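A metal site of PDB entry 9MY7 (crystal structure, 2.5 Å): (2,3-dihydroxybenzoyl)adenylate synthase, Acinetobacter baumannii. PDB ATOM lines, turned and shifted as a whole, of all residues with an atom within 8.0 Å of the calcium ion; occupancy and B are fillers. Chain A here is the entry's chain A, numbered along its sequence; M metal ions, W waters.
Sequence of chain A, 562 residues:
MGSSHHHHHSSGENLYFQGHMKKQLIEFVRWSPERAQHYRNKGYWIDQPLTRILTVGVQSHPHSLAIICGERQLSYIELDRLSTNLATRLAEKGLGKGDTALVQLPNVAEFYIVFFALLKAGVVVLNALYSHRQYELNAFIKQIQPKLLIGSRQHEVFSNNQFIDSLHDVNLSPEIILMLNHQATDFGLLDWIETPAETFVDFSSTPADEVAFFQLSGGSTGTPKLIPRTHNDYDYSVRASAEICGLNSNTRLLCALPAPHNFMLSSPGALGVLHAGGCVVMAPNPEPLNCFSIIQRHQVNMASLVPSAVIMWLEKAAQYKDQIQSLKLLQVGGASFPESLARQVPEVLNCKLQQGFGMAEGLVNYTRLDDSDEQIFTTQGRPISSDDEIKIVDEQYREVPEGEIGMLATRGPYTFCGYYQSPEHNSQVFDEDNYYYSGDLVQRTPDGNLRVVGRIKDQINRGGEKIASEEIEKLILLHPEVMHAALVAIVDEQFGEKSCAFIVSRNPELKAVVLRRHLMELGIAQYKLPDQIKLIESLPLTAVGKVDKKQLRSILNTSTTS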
ATOM      1  N   VAL A 300      10.310   9.123 -25.565  1.00  0.00           N
ATOM      2  CA  VAL A 300      11.051   9.106 -24.311  1.00  0.00           C
ATOM      3  C   VAL A 300      10.108   8.718 -23.187  1.00  0.00           C
ATOM      4  O   VAL A 300       8.986   9.242 -23.076  1.00  0.00           O
ATOM      5  CB  VAL A 300      11.684  10.485 -24.053  1.00  0.00           C
ATOM      6  CG1 VAL A 300      11.906  10.686 -22.560  1.00  0.00           C
ATOM      7  CG2 VAL A 300      12.974  10.638 -24.855  1.00  0.00           C
ATOM      8  N   ASN A 301      10.542   7.774 -22.356  1.00  0.00           N
ATOM      9  CA  ASN A 301       9.721   7.310 -21.248  1.00  0.00           C
ATOM     10  C   ASN A 301      10.231   7.771 -19.889  1.00  0.00           C
ATOM     11  O   ASN A 301       9.525   7.580 -18.894  1.00  0.00           O
ATOM     12  CB  ASN A 301       9.643   5.775 -21.229  1.00  0.00           C
ATOM     13  CG  ASN A 301      10.960   5.107 -21.545  1.00  0.00           C
ATOM     14  OD1 ASN A 301      11.963   5.335 -20.876  1.00  0.00           O
ATOM     15  ND2 ASN A 301      10.966   4.268 -22.573  1.00  0.00           N
ATOM     16  N   LYS A 321       0.078  18.189 -23.596  1.00  0.00           N
ATOM     17  CA  LYS A 321       0.009  16.923 -22.866  1.00  0.00           C
ATOM     18  C   LYS A 321       0.368  15.746 -23.772  1.00  0.00           C
ATOM     19  O   LYS A 321       1.092  14.836 -23.352  1.00  0.00           O
ATOM     20  CB  LYS A 321      -1.385  16.729 -22.272  1.00  0.00           C
ATOM     21  CG  LYS A 321      -1.473  17.050 -20.791  1.00  0.00           C
ATOM     22  CD  LYS A 321      -2.722  16.424 -20.178  1.00  0.00           C
ATOM     23  N   ILE A 324       4.149  14.773 -24.524  1.00  0.00           N
ATOM     24  CA  ILE A 324       4.930  14.130 -23.468  1.00  0.00           C
ATOM     25  C   ILE A 324       4.158  12.986 -22.815  1.00  0.00           C
ATOM     26  O   ILE A 324       4.465  12.605 -21.690  1.00  0.00           O
ATOM     27  CB  ILE A 324       5.393  15.155 -22.418  1.00  0.00           C
ATOM     28  CG1 ILE A 324       4.189  15.697 -21.632  1.00  0.00           C
ATOM     29  CG2 ILE A 324       6.167  16.288 -23.084  1.00  0.00           C
ATOM     30  CD1 ILE A 324       4.504  16.019 -20.180  1.00  0.00           C
ATOM     31  N   GLN A 325       3.176  12.419 -23.498  1.00  0.00           N
ATOM     32  CA  GLN A 325       2.424  11.315 -22.914  1.00  0.00           C
ATOM     33  C   GLN A 325       3.313  10.094 -22.689  1.00  0.00           C
ATOM     34  O   GLN A 325       3.076   9.330 -21.753  1.00  0.00           O
ATOM     35  CB  GLN A 325       1.232  10.951 -23.804  1.00  0.00           C
ATOM     36  CG  GLN A 325       1.608  10.512 -25.213  1.00  0.00           C
ATOM     37  CD  GLN A 325       1.823   9.019 -25.328  1.00  0.00           C
ATOM     38  OE1 GLN A 325       1.079   8.228 -24.740  1.00  0.00           O
ATOM     39  NE2 GLN A 325       2.844   8.617 -26.072  1.00  0.00           N
ATOM     40  N   SER A 326       4.336   9.909 -23.520  1.00  0.00           N
ATOM     41  CA  SER A 326       5.178   8.723 -23.417  1.00  0.00           C
ATOM     42  C   SER A 326       6.001   8.700 -22.141  1.00  0.00           C
ATOM     43  O   SER A 326       6.539   7.644 -21.781  1.00  0.00           O
ATOM     44  CB  SER A 326       6.100   8.625 -24.629  1.00  0.00           C
ATOM     45  OG  SER A 326       6.844   9.814 -24.813  1.00  0.00           O
ATOM     46  N   LEU A 327       6.123   9.829 -21.446  1.00  0.00           N
ATOM     47  CA  LEU A 327       6.883   9.845 -20.197  1.00  0.00           C
ATOM     48  C   LEU A 327       6.199   8.976 -19.148  1.00  0.00           C
ATOM     49  O   LEU A 327       4.982   9.042 -18.972  1.00  0.00           O
ATOM     50  CB  LEU A 327       7.016  11.279 -19.687  1.00  0.00           C
ATOM     51  N   LYS A 328       6.989   8.151 -18.471  1.00  0.00           N
ATOM     52  CA  LYS A 328       6.476   7.266 -17.435  1.00  0.00           C
ATOM     53  C   LYS A 328       7.075   7.520 -16.059  1.00  0.00           C
ATOM     54  O   LYS A 328       6.436   7.183 -15.052  1.00  0.00           O
ATOM     55  CB  LYS A 328       6.705   5.794 -17.802  1.00  0.00           C
ATOM     56  N   LEU A 329       8.274   8.095 -15.970  1.00  0.00           N
ATOM     57  CA  LEU A 329       8.918   8.343 -14.682  1.00  0.00           C
ATOM     58  C   LEU A 329       9.816   9.564 -14.801  1.00  0.00           C
ATOM     59  O   LEU A 329      10.628   9.643 -15.730  1.00  0.00           O
ATOM     60  CB  LEU A 329       9.726   7.123 -14.227  1.00  0.00           C
ATOM     61  CG  LEU A 329      10.521   7.279 -12.930  1.00  0.00           C
ATOM     62  CD1 LEU A 329       9.590   7.454 -11.747  1.00  0.00           C
ATOM     63  CD2 LEU A 329      11.435   6.083 -12.711  1.00  0.00           C
ATOM     64  N   PRO A 346       2.403  14.064 -11.215  1.00  0.00           N
ATOM     65  CA  PRO A 346       1.509  13.010 -11.727  1.00  0.00           C
ATOM     66  C   PRO A 346       0.241  13.554 -12.362  1.00  0.00           C
ATOM     67  O   PRO A 346      -0.214  13.019 -13.380  1.00  0.00           O
ATOM     68  CB  PRO A 346       1.194  12.173 -10.476  1.00  0.00           C
ATOM     69  CG  PRO A 346       1.578  13.030  -9.310  1.00  0.00           C
ATOM     70  CD  PRO A 346       2.673  13.940  -9.779  1.00  0.00           C
ATOM     71  N   LEU A 349       1.897  16.319 -15.464  1.00  0.00           N
ATOM     72  CA  LEU A 349       2.829  15.664 -16.366  1.00  0.00           C
ATOM     73  C   LEU A 349       2.449  14.227 -16.683  1.00  0.00           C
ATOM     74  O   LEU A 349       3.012  13.636 -17.610  1.00  0.00           O
ATOM     75  CB  LEU A 349       4.244  15.711 -15.788  1.00  0.00           C
ATOM     76  CG  LEU A 349       4.883  17.101 -15.755  1.00  0.00           C
ATOM     77  CD1 LEU A 349       6.277  17.057 -15.150  1.00  0.00           C
ATOM     78  CD2 LEU A 349       4.918  17.723 -17.150  1.00  0.00           C
ATOM     79  N   ASN A 350       1.510  13.636 -15.926  1.00  0.00           N
ATOM     80  CA  ASN A 350       0.979  12.304 -16.226  1.00  0.00           C
ATOM     81  C   ASN A 350       2.081  11.253 -16.243  1.00  0.00           C
ATOM     82  O   ASN A 350       2.142  10.398 -17.142  1.00  0.00           O
ATOM     83  CB  ASN A 350       0.194  12.311 -17.540  1.00  0.00           C
ATOM     84  CG  ASN A 350      -1.084  13.118 -17.450  1.00  0.00           C
ATOM     85  OD1 ASN A 350      -1.932  12.871 -16.601  1.00  0.00           O
ATOM     86  ND2 ASN A 350      -1.219  14.103 -18.325  1.00  0.00           N
ATOM     87  N   CYS A 351       2.968  11.314 -15.249  1.00  0.00           N
ATOM     88  CA  CYS A 351       3.997  10.300 -15.055  1.00  0.00           C
ATOM     89  C   CYS A 351       4.254  10.201 -13.559  1.00  0.00           C
ATOM     90  O   CYS A 351       3.805  11.038 -12.776  1.00  0.00           O
ATOM     91  CB  CYS A 351       5.276  10.634 -15.818  1.00  0.00           C
ATOM     92  SG  CYS A 351       6.015  12.224 -15.368  1.00  0.00           S
ATOM     93  N   LYS A 352       4.981   9.158 -13.163  1.00  0.00           N
ATOM     94  CA  LYS A 352       5.300   9.014 -11.753  1.00  0.00           C
ATOM     95  C   LYS A 352       6.556   9.818 -11.415  1.00  0.00           C
ATOM     96  O   LYS A 352       7.399  10.101 -12.262  1.00  0.00           O
ATOM     97  CB  LYS A 352       5.487   7.551 -11.372  1.00  0.00           C
ATOM     98  CG  LYS A 352       5.402   7.330  -9.862  1.00  0.00           C
ATOM     99  CD  LYS A 352       4.632   8.483  -9.222  1.00  0.00           C
ATOM    100  CE  LYS A 352       4.526   8.353  -7.718  1.00  0.00           C
ATOM    101  NZ  LYS A 352       3.521   9.301  -7.162  1.00  0.00           N
HETATM  102 CA    CA M   1       2.675   9.137 -19.367  1.00  0.00          CA
HETATM  103  O   HOH W   1       1.929   7.840 -17.072  1.00  0.00           O
HETATM  104  O   HOH W   2       3.015  11.404 -19.822  1.00  0.00           O
HETATM  105  O   HOH W   3       1.572   6.872 -19.761  1.00  0.00           O
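The nearest printed residue that does not touch the calcium ion is Ser 326 (4.4 Å).
Water W2 binds the calcium ion (2.3 Å). O of Leu 327 is bound to the calcium ion (2.3 Å). O of Gln 325 binds the calcium ion (2.4 Å). The calcium ion is bound by water W3. O of Asn 350 is bound to the calcium ion, at 2.6 Å. The calcium ion is bound by water W1. The calcium ion has six donor atoms within binding distance.
The backbone carbonyl oxygen (O) of Val 300 sits at hydrogen-bond distance from the backbone NH (N) of Leu 327, 3.3 Å away.
Water W2 bridges the backbone carbonyl oxygen of Ile 324 and the backbone carbonyl oxygen of Leu 349.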
